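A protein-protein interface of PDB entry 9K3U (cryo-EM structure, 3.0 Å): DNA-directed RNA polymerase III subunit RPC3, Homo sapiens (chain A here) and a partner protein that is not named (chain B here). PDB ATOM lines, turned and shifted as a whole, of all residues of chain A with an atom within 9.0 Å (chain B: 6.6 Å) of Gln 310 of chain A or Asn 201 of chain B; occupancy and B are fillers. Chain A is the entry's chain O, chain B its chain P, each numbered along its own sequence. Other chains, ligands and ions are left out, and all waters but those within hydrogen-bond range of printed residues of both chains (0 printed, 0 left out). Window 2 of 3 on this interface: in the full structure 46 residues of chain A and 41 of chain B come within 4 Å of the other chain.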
ATOM      1  N   THR A 262     -16.922  -2.121 -15.764  1.00  0.00           N
ATOM      2  CA  THR A 262     -17.287  -1.822 -14.382  1.00  0.00           C
ATOM      3  C   THR A 262     -17.837  -3.060 -13.683  1.00  0.00           C
ATOM      4  O   THR A 262     -17.438  -3.375 -12.555  1.00  0.00           O
ATOM      5  CB  THR A 262     -18.313  -0.688 -14.343  1.00  0.00           C
ATOM      6  OG1 THR A 262     -19.475  -1.064 -15.092  1.00  0.00           O
ATOM      7  CG2 THR A 262     -17.720   0.586 -14.932  1.00  0.00           C
ATOM      8  N   SER A 263     -18.756  -3.772 -14.339  1.00  0.00           N
ATOM      9  CA  SER A 263     -19.265  -5.017 -13.777  1.00  0.00           C
ATOM     10  C   SER A 263     -18.145  -6.036 -13.607  1.00  0.00           C
ATOM     11  O   SER A 263     -18.140  -6.812 -12.644  1.00  0.00           O
ATOM     12  CB  SER A 263     -20.372  -5.577 -14.669  1.00  0.00           C
ATOM     13  OG  SER A 263     -20.840  -6.824 -14.185  1.00  0.00           O
ATOM     14  N   ILE A 266     -16.324  -5.118 -10.486  1.00  0.00           N
ATOM     15  CA  ILE A 266     -17.151  -5.429  -9.323  1.00  0.00           C
ATOM     16  C   ILE A 266     -17.092  -6.922  -9.017  1.00  0.00           C
ATOM     17  O   ILE A 266     -16.904  -7.332  -7.864  1.00  0.00           O
ATOM     18  CB  ILE A 266     -18.599  -4.956  -9.547  1.00  0.00           C
ATOM     19  CG1 ILE A 266     -18.665  -3.424  -9.598  1.00  0.00           C
ATOM     20  CG2 ILE A 266     -19.515  -5.499  -8.461  1.00  0.00           C
ATOM     21  CD1 ILE A 266     -18.266  -2.731  -8.304  1.00  0.00           C
ATOM     22  N   SER A 290     -23.569  -4.768   0.201  1.00  0.00           N
ATOM     23  CA  SER A 290     -23.196  -3.614  -0.608  1.00  0.00           C
ATOM     24  C   SER A 290     -22.187  -2.726   0.109  1.00  0.00           C
ATOM     25  O   SER A 290     -21.260  -2.216  -0.525  1.00  0.00           O
ATOM     26  CB  SER A 290     -24.442  -2.807  -0.975  1.00  0.00           C
ATOM     27  OG  SER A 290     -25.138  -2.386   0.186  1.00  0.00           O
ATOM     28  N   ILE A 303     -17.041   5.743  -8.274  1.00  0.00           N
ATOM     29  CA  ILE A 303     -18.333   5.070  -8.212  1.00  0.00           C
ATOM     30  C   ILE A 303     -18.942   5.334  -6.843  1.00  0.00           C
ATOM     31  O   ILE A 303     -18.230   5.351  -5.834  1.00  0.00           O
ATOM     32  CB  ILE A 303     -18.201   3.555  -8.467  1.00  0.00           C
ATOM     33  CG1 ILE A 303     -19.561   2.869  -8.324  1.00  0.00           C
ATOM     34  CG2 ILE A 303     -17.186   2.937  -7.515  1.00  0.00           C
ATOM     35  CD1 ILE A 303     -19.579   1.437  -8.812  1.00  0.00           C
ATOM     36  N   SER A 304     -20.258   5.537  -6.812  1.00  0.00           N
ATOM     37  CA  SER A 304     -20.971   5.864  -5.591  1.00  0.00           C
ATOM     38  C   SER A 304     -21.795   4.665  -5.126  1.00  0.00           C
ATOM     39  O   SER A 304     -21.917   3.649  -5.823  1.00  0.00           O
ATOM     40  CB  SER A 304     -21.846   7.099  -5.816  1.00  0.00           C
ATOM     41  OG  SER A 304     -22.789   6.874  -6.848  1.00  0.00           O
ATOM     42  N   LYS A 305     -22.379   4.781  -3.931  1.00  0.00           N
ATOM     43  CA  LYS A 305     -23.168   3.687  -3.377  1.00  0.00           C
ATOM     44  C   LYS A 305     -24.396   3.404  -4.233  1.00  0.00           C
ATOM     45  O   LYS A 305     -24.746   2.238  -4.457  1.00  0.00           O
ATOM     46  CB  LYS A 305     -23.579   4.016  -1.941  1.00  0.00           C
ATOM     47  CG  LYS A 305     -24.360   2.914  -1.235  1.00  0.00           C
ATOM     48  CD  LYS A 305     -23.524   1.655  -1.066  1.00  0.00           C
ATOM     49  CE  LYS A 305     -24.260   0.606  -0.246  1.00  0.00           C
ATOM     50  NZ  LYS A 305     -25.537   0.188  -0.885  1.00  0.00           N
ATOM     51  N   GLN A 306     -25.062   4.452  -4.723  1.00  0.00           N
ATOM     52  CA  GLN A 306     -26.234   4.240  -5.568  1.00  0.00           C
ATOM     53  C   GLN A 306     -25.851   3.606  -6.899  1.00  0.00           C
ATOM     54  O   GLN A 306     -26.584   2.750  -7.407  1.00  0.00           O
ATOM     55  CB  GLN A 306     -26.967   5.566  -5.786  1.00  0.00           C
ATOM     56  CG  GLN A 306     -26.168   6.618  -6.542  1.00  0.00           C
ATOM     57  CD  GLN A 306     -26.416   6.586  -8.039  1.00  0.00           C
ATOM     58  OE1 GLN A 306     -27.056   5.671  -8.557  1.00  0.00           O
ATOM     59  NE2 GLN A 306     -25.912   7.594  -8.740  1.00  0.00           N
ATOM     60  N   VAL A 307     -24.709   3.994  -7.470  1.00  0.00           N
ATOM     61  CA  VAL A 307     -24.260   3.369  -8.710  1.00  0.00           C
ATOM     62  C   VAL A 307     -23.944   1.897  -8.476  1.00  0.00           C
ATOM     63  O   VAL A 307     -24.268   1.038  -9.307  1.00  0.00           O
ATOM     64  CB  VAL A 307     -23.042   4.121  -9.282  1.00  0.00           C
ATOM     65  CG1 VAL A 307     -22.557   3.452 -10.558  1.00  0.00           C
ATOM     66  CG2 VAL A 307     -23.382   5.583  -9.545  1.00  0.00           C
ATOM     67  N   LEU A 308     -23.306   1.579  -7.350  1.00  0.00           N
ATOM     68  CA  LEU A 308     -23.023   0.182  -7.034  1.00  0.00           C
ATOM     69  C   LEU A 308     -24.312  -0.609  -6.850  1.00  0.00           C
ATOM     70  O   LEU A 308     -24.416  -1.753  -7.314  1.00  0.00           O
ATOM     71  CB  LEU A 308     -22.157   0.094  -5.778  1.00  0.00           C
ATOM     72  CG  LEU A 308     -21.813  -1.319  -5.293  1.00  0.00           C
ATOM     73  CD1 LEU A 308     -21.071  -2.098  -6.368  1.00  0.00           C
ATOM     74  CD2 LEU A 308     -20.993  -1.257  -4.013  1.00  0.00           C
ATOM     75  N   ASP A 309     -25.302  -0.021  -6.177  1.00  0.00           N
ATOM     76  CA  ASP A 309     -26.578  -0.704  -5.997  1.00  0.00           C
ATOM     77  C   ASP A 309     -27.261  -0.943  -7.338  1.00  0.00           C
ATOM     78  O   ASP A 309     -27.844  -2.010  -7.566  1.00  0.00           O
ATOM     79  CB  ASP A 309     -27.481   0.113  -5.070  1.00  0.00           C
ATOM     80  CG  ASP A 309     -28.688  -0.670  -4.585  1.00  0.00           C
ATOM     81  OD1 ASP A 309     -29.153  -1.572  -5.313  1.00  0.00           O
ATOM     82  OD2 ASP A 309     -29.170  -0.386  -3.468  1.00  0.00           O
ATOM     83  N   GLN A 310     -27.204   0.042  -8.236  1.00  0.00           N
ATOM     84  CA  GLN A 310     -27.780  -0.135  -9.566  1.00  0.00           C
ATOM     85  C   GLN A 310     -27.078  -1.256 -10.321  1.00  0.00           C
ATOM     86  O   GLN A 310     -27.731  -2.099 -10.949  1.00  0.00           O
ATOM     87  CB  GLN A 310     -27.701   1.174 -10.352  1.00  0.00           C
ATOM     88  CG  GLN A 310     -28.647   2.253  -9.848  1.00  0.00           C
ATOM     89  CD  GLN A 310     -28.535   3.541 -10.639  1.00  0.00           C
ATOM     90  OE1 GLN A 310     -27.736   3.646 -11.569  1.00  0.00           O
ATOM     91  NE2 GLN A 310     -29.341   4.532 -10.272  1.00  0.00           N
ATOM     92  N   TYR A 311     -25.744  -1.282 -10.274  1.00  0.00           N
ATOM     93  CA  TYR A 311     -25.001  -2.356 -10.927  1.00  0.00           C
ATOM     94  C   TYR A 311     -25.407  -3.714 -10.368  1.00  0.00           C
ATOM     95  O   TYR A 311     -25.638  -4.665 -11.122  1.00  0.00           O
ATOM     96  CB  TYR A 311     -23.497  -2.137 -10.761  1.00  0.00           C
ATOM     97  CG  TYR A 311     -22.908  -1.041 -11.630  1.00  0.00           C
ATOM     98  CD1 TYR A 311     -23.412  -0.776 -12.897  1.00  0.00           C
ATOM     99  CD2 TYR A 311     -21.841  -0.273 -11.180  1.00  0.00           C
ATOM    100  CE1 TYR A 311     -22.872   0.219 -13.689  1.00  0.00           C
ATOM    101  CE2 TYR A 311     -21.294   0.722 -11.965  1.00  0.00           C
ATOM    102  CZ  TYR A 311     -21.814   0.966 -13.217  1.00  0.00           C
ATOM    103  OH  TYR A 311     -21.274   1.960 -14.000  1.00  0.00           O
ATOM    104  N   LEU A 312     -25.502  -3.821  -9.042  1.00  0.00           N
ATOM    105  CA  LEU A 312     -25.843  -5.103  -8.433  1.00  0.00           C
ATOM    106  C   LEU A 312     -27.253  -5.543  -8.815  1.00  0.00           C
ATOM    107  O   LEU A 312     -27.471  -6.710  -9.162  1.00  0.00           O
ATOM    108  CB  LEU A 312     -25.703  -5.014  -6.912  1.00  0.00           C
ATOM    109  CG  LEU A 312     -24.278  -4.824  -6.383  1.00  0.00           C
ATOM    110  CD1 LEU A 312     -24.292  -4.610  -4.877  1.00  0.00           C
ATOM    111  CD2 LEU A 312     -23.399  -6.013  -6.744  1.00  0.00           C
ATOM    112  N   THR A 313     -28.222  -4.624  -8.769  1.00  0.00           N
ATOM    113  CA  THR A 313     -29.599  -4.996  -9.067  1.00  0.00           C
ATOM    114  C   THR A 313     -29.820  -5.263 -10.549  1.00  0.00           C
ATOM    115  O   THR A 313     -30.741  -6.012 -10.896  1.00  0.00           O
ATOM    116  CB  THR A 313     -30.565  -3.911  -8.586  1.00  0.00           C
ATOM    117  OG1 THR A 313     -31.916  -4.366  -8.739  1.00  0.00           O
ATOM    118  CG2 THR A 313     -30.383  -2.630  -9.380  1.00  0.00           C
ATOM    119  N   LEU A 314     -29.012  -4.675 -11.434  1.00  0.00           N
ATOM    120  CA  LEU A 314     -29.122  -4.993 -12.852  1.00  0.00           C
ATOM    121  C   LEU A 314     -28.371  -6.265 -13.215  1.00  0.00           C
ATOM    122  O   LEU A 314     -28.740  -6.939 -14.184  1.00  0.00           O
ATOM    123  CB  LEU A 314     -28.619  -3.822 -13.704  1.00  0.00           C
ATOM    124  CG  LEU A 314     -27.112  -3.635 -13.920  1.00  0.00           C
ATOM    125  CD1 LEU A 314     -26.616  -4.410 -15.136  1.00  0.00           C
ATOM    126  CD2 LEU A 314     -26.788  -2.156 -14.070  1.00  0.00           C
ATOM    127  N   LEU A 315     -27.326  -6.614 -12.457  1.00  0.00           N
ATOM    128  CA  LEU A 315     -26.694  -7.918 -12.635  1.00  0.00           C
ATOM    129  C   LEU A 315     -27.588  -9.039 -12.122  1.00  0.00           C
ATOM    130  O   LEU A 315     -27.638 -10.116 -12.723  1.00  0.00           O
ATOM    131  CB  LEU A 315     -25.347  -7.956 -11.918  1.00  0.00           C
ATOM    132  CG  LEU A 315     -24.098  -7.730 -12.772  1.00  0.00           C
ATOM    133  CD1 LEU A 315     -24.080  -6.329 -13.362  1.00  0.00           C
ATOM    134  CD2 LEU A 315     -22.847  -7.985 -11.943  1.00  0.00           C
ATOM    135  N   ALA A 316     -28.297  -8.804 -11.012  1.00  0.00           N
ATOM    136  CA  ALA A 316     -29.193  -9.826 -10.483  1.00  0.00           C
ATOM    137  C   ALA A 316     -30.312 -10.156 -11.465  1.00  0.00           C
ATOM    138  O   ALA A 316     -30.812 -11.286 -11.471  1.00  0.00           O
ATOM    139  CB  ALA A 316     -29.778  -9.368  -9.148  1.00  0.00           C
ATOM    140  N   ASP A 317     -30.712  -9.193 -12.291  1.00  0.00           N
ATOM    141  CA  ASP A 317     -31.753  -9.399 -13.288  1.00  0.00           C
ATOM    142  C   ASP A 317     -31.210  -9.954 -14.599  1.00  0.00           C
ATOM    143  O   ASP A 317     -31.969 -10.087 -15.565  1.00  0.00           O
ATOM    144  CB  ASP A 317     -32.492  -8.085 -13.552  1.00  0.00           C
ATOM    145  CG  ASP A 317     -33.147  -7.523 -12.306  1.00  0.00           C
ATOM    146  OD1 ASP A 317     -33.537  -8.320 -11.426  1.00  0.00           O
ATOM    147  OD2 ASP A 317     -33.273  -6.284 -12.206  1.00  0.00           O
ATOM    148  N   TYR A 334     -25.986  -9.707  -1.849  1.00  0.00           N
ATOM    149  CA  TYR A 334     -25.947 -10.438  -3.107  1.00  0.00           C
ATOM    150  C   TYR A 334     -24.966 -11.596  -2.995  1.00  0.00           C
ATOM    151  O   TYR A 334     -24.082 -11.609  -2.132  1.00  0.00           O
ATOM    152  CB  TYR A 334     -25.552  -9.525  -4.277  1.00  0.00           C
ATOM    153  CG  TYR A 334     -26.600  -8.489  -4.621  1.00  0.00           C
ATOM    154  CD1 TYR A 334     -26.680  -7.293  -3.922  1.00  0.00           C
ATOM    155  CD2 TYR A 334     -27.509  -8.708  -5.647  1.00  0.00           C
ATOM    156  CE1 TYR A 334     -27.635  -6.344  -4.233  1.00  0.00           C
ATOM    157  CE2 TYR A 334     -28.469  -7.766  -5.967  1.00  0.00           C
ATOM    158  CZ  TYR A 334     -28.526  -6.586  -5.256  1.00  0.00           C
ATOM    159  OH  TYR A 334     -29.480  -5.644  -5.568  1.00  0.00           O
ATOM    160  N   ALA B 195     -26.085   4.274 -26.898  1.00  0.00           N
ATOM    161  CA  ALA B 195     -26.368   4.155 -25.473  1.00  0.00           C
ATOM    162  C   ALA B 195     -25.084   4.133 -24.657  1.00  0.00           C
ATOM    163  O   ALA B 195     -24.991   4.784 -23.610  1.00  0.00           O
ATOM    164  CB  ALA B 195     -27.192   2.893 -25.206  1.00  0.00           C
ATOM    165  N   SER B 198     -23.538   7.609 -24.577  1.00  0.00           N
ATOM    166  CA  SER B 198     -24.248   8.569 -23.741  1.00  0.00           C
ATOM    167  C   SER B 198     -23.667   8.611 -22.332  1.00  0.00           C
ATOM    168  O   SER B 198     -23.491   9.693 -21.760  1.00  0.00           O
ATOM    169  CB  SER B 198     -25.738   8.227 -23.694  1.00  0.00           C
ATOM    170  OG  SER B 198     -25.952   6.973 -23.074  1.00  0.00           O
ATOM    171  N   LYS B 199     -23.359   7.443 -21.765  1.00  0.00           N
ATOM    172  CA  LYS B 199     -22.753   7.322 -20.441  1.00  0.00           C
ATOM    173  C   LYS B 199     -23.378   8.273 -19.426  1.00  0.00           C
ATOM    174  O   LYS B 199     -22.667   8.919 -18.650  1.00  0.00           O
ATOM    175  CB  LYS B 199     -21.240   7.559 -20.520  1.00  0.00           C
ATOM    176  CG  LYS B 199     -20.819   8.945 -20.995  1.00  0.00           C
ATOM    177  CD  LYS B 199     -19.312   9.122 -20.899  1.00  0.00           C
ATOM    178  CE  LYS B 199     -18.886  10.528 -21.287  1.00  0.00           C
ATOM    179  NZ  LYS B 199     -19.444  11.557 -20.368  1.00  0.00           N
ATOM    180  N   GLN B 200     -24.710   8.360 -19.419  1.00  0.00           N
ATOM    181  CA  GLN B 200     -25.395   9.224 -18.463  1.00  0.00           C
ATOM    182  C   GLN B 200     -25.660   8.492 -17.148  1.00  0.00           C
ATOM    183  O   GLN B 200     -25.484   9.060 -16.066  1.00  0.00           O
ATOM    184  CB  GLN B 200     -26.703   9.740 -19.070  1.00  0.00           C
ATOM    185  CG  GLN B 200     -27.395  10.827 -18.255  1.00  0.00           C
ATOM    186  CD  GLN B 200     -28.238  10.272 -17.123  1.00  0.00           C
ATOM    187  OE1 GLN B 200     -28.565   9.087 -17.099  1.00  0.00           O
ATOM    188  NE2 GLN B 200     -28.598  11.134 -16.180  1.00  0.00           N
ATOM    189  N   ASN B 201     -26.086   7.228 -17.231  1.00  0.00           N
ATOM    190  CA  ASN B 201     -26.374   6.418 -16.056  1.00  0.00           C
ATOM    191  C   ASN B 201     -26.549   4.988 -16.532  1.00  0.00           C
ATOM    192  O   ASN B 201     -27.010   4.790 -17.663  1.00  0.00           O
ATOM    193  CB  ASN B 201     -27.637   6.908 -15.335  1.00  0.00           C
ATOM    194  CG  ASN B 201     -27.919   6.142 -14.060  1.00  0.00           C
ATOM    195  OD1 ASN B 201     -27.346   6.431 -13.010  1.00  0.00           O
ATOM    196  ND2 ASN B 201     -28.810   5.161 -14.144  1.00  0.00           N
ATOM    197  N   PRO B 202     -26.185   3.976 -15.737  1.00  0.00           N
ATOM    198  CA  PRO B 202     -26.309   2.593 -16.235  1.00  0.00           C
ATOM    199  C   PRO B 202     -27.722   2.217 -16.647  1.00  0.00           C
ATOM    200  O   PRO B 202     -27.918   1.618 -17.715  1.00  0.00           O
ATOM    201  CB  PRO B 202     -25.815   1.751 -15.051  1.00  0.00           C
ATOM    202  CG  PRO B 202     -24.923   2.662 -14.284  1.00  0.00           C
ATOM    203  CD  PRO B 202     -25.528   4.027 -14.418  1.00  0.00           C
ATOM    204  N   MET B 203     -28.720   2.544 -15.823  1.00  0.00           N
ATOM    205  CA  MET B 203     -30.095   2.180 -16.151  1.00  0.00           C
ATOM    206  C   MET B 203     -30.567   2.886 -17.413  1.00  0.00           C
ATOM    207  O   MET B 203     -31.222   2.275 -18.267  1.00  0.00           O
ATOM    208  CB  MET B 203     -31.018   2.511 -14.978  1.00  0.00           C
ATOM    209  CG  MET B 203     -30.717   1.721 -13.712  1.00  0.00           C
ATOM    210  SD  MET B 203     -30.980  -0.051 -13.916  1.00  0.00           S
ATOM    211  CE  MET B 203     -30.535  -0.652 -12.287  1.00  0.00           C
ATOM    212  N   ILE B 204     -30.248   4.173 -17.553  1.00  0.00           N
ATOM    213  CA  ILE B 204     -30.647   4.909 -18.749  1.00  0.00           C
ATOM    214  C   ILE B 204     -29.954   4.338 -19.980  1.00  0.00           C
ATOM    215  O   ILE B 204     -30.555   4.223 -21.052  1.00  0.00           O
ATOM    216  CB  ILE B 204     -30.355   6.413 -18.577  1.00  0.00           C
ATOM    217  CG1 ILE B 204     -31.434   7.082 -17.721  1.00  0.00           C
ATOM    218  CG2 ILE B 204     -30.263   7.106 -19.931  1.00  0.00           C
ATOM    219  CD1 ILE B 204     -31.532   6.544 -16.307  1.00  0.00           C
ATOM    220  N   GLN B 205     -28.679   3.967 -19.840  1.00  0.00           N
ATOM    221  CA  GLN B 205     -27.958   3.360 -20.954  1.00  0.00           C
ATOM    222  C   GLN B 205     -28.609   2.053 -21.379  1.00  0.00           C
ATOM    223  O   GLN B 205     -28.774   1.794 -22.577  1.00  0.00           O
ATOM    224  CB  GLN B 205     -26.497   3.124 -20.568  1.00  0.00           C
ATOM    225  CG  GLN B 205     -25.686   4.392 -20.374  1.00  0.00           C
ATOM    226  CD  GLN B 205     -24.352   4.130 -19.702  1.00  0.00           C
ATOM    227  OE1 GLN B 205     -23.991   4.798 -18.732  1.00  0.00           O
ATOM    228  NE2 GLN B 205     -23.614   3.154 -20.215  1.00  0.00           N
ATOM    229  N   ARG B 206     -28.982   1.211 -20.413  1.00  0.00           N
ATOM    230  CA  ARG B 206     -29.636  -0.047 -20.757  1.00  0.00           C
ATOM    231  C   ARG B 206     -30.988   0.196 -21.414  1.00  0.00           C
ATOM    232  O   ARG B 206     -31.329  -0.458 -22.410  1.00  0.00           O
ATOM    233  CB  ARG B 206     -29.793  -0.916 -19.508  1.00  0.00           C
ATOM    234  CG  ARG B 206     -28.478  -1.354 -18.871  1.00  0.00           C
ATOM    235  CD  ARG B 206     -27.642  -2.217 -19.808  1.00  0.00           C
ATOM    236  NE  ARG B 206     -28.361  -3.409 -20.254  1.00  0.00           N
ATOM    237  CZ  ARG B 206     -28.388  -4.567 -19.598  1.00  0.00           C
ATOM    238  NH1 ARG B 206     -27.737  -4.706 -18.448  1.00  0.00           N
ATOM    239  NH2 ARG B 206     -29.070  -5.589 -20.091  1.00  0.00           N
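The side-chain amide oxygen (OE1) of Gln 310 of chain A lies close to the side-chain amide oxygen (OD1) of Asn 201 of chain B, at 3.2 Å.
NE2 of Gln 310 of chain A is in hydrogen-bond range of OE1 of Gln 306 of chain A (3.1 Å). ND2 of Asn 201 of chain B sits close to N of Met 203 of chain B, at 3.1 Å. The backbone carbonyl oxygen of Asn 201 of chain B lies close to the side-chain amide oxygen of Gln 205 of chain B (3.2 Å).
Among the printed residues, pairs that only touch across the chains: Tyr 311 of chain A with Pro 202 of chain B (3.2 Å), Gln 310 of chain A with Met 203 of chain B (3.4 Å), Leu 314 of chain A with Arg 206 of chain B (3.5 Å), Thr 313 of chain A with Met 203 of chain B (3.5 Å), Gln 310 of chain A with Pro 202 of chain B (3.6 Å) and Leu 314 of chain A with Met 203 of chain B (3.97 Å).
Of the printed residues of chain B, Gln 310 of chain A touches Asn 201 (3.2 Å), Pro 202 (3.6 Å) and Met 203 (3.4 Å). Asn 201 of chain B touches just one residue of chain A: Gln 310 (3.2 Å). No residue of chain A comes within 4 Å of Gln 200 of chain B. No residue of chain A comes within 4 Å of Ile 204 of chain B. Of the printed residues of chain B, Tyr 311 of chain A touches Pro 202. Printed residues of chain A within 4 Å of Arg 206 of chain B: Leu 314. Ala 195 of chain B touches none of the printed residues of chain A. The nearest residue of chain B that does not touch Gln 310 of chain A is Ile 204 of chain B (6.5 Å). The nearest printed residue of chain B that does not touch Thr 313 of chain A is Arg 206 of chain B (8.2 Å).
Printed residues of chain A that touch a printed residue of chain B: Gln 310, Tyr 311, Thr 313 and Leu 314. Hydrophobic or aromatic side chains of chain A within 4 Å of the printed part of chain B: Tyr 311 and Leu 314. Of the 10 printed residues of chain B, 4 touch a printed residue of chain A. Hydrophobic or aromatic side chains of chain B that line the printed part of chain A: Pro 202 and Met 203. Along chain B the printed residues that touch a printed residue of chain A span positions 201 to 206. Among the printed residues, no Asp or Glu carboxylate lies within 4 Å of a Lys or Arg side-chain nitrogen of the other chain.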
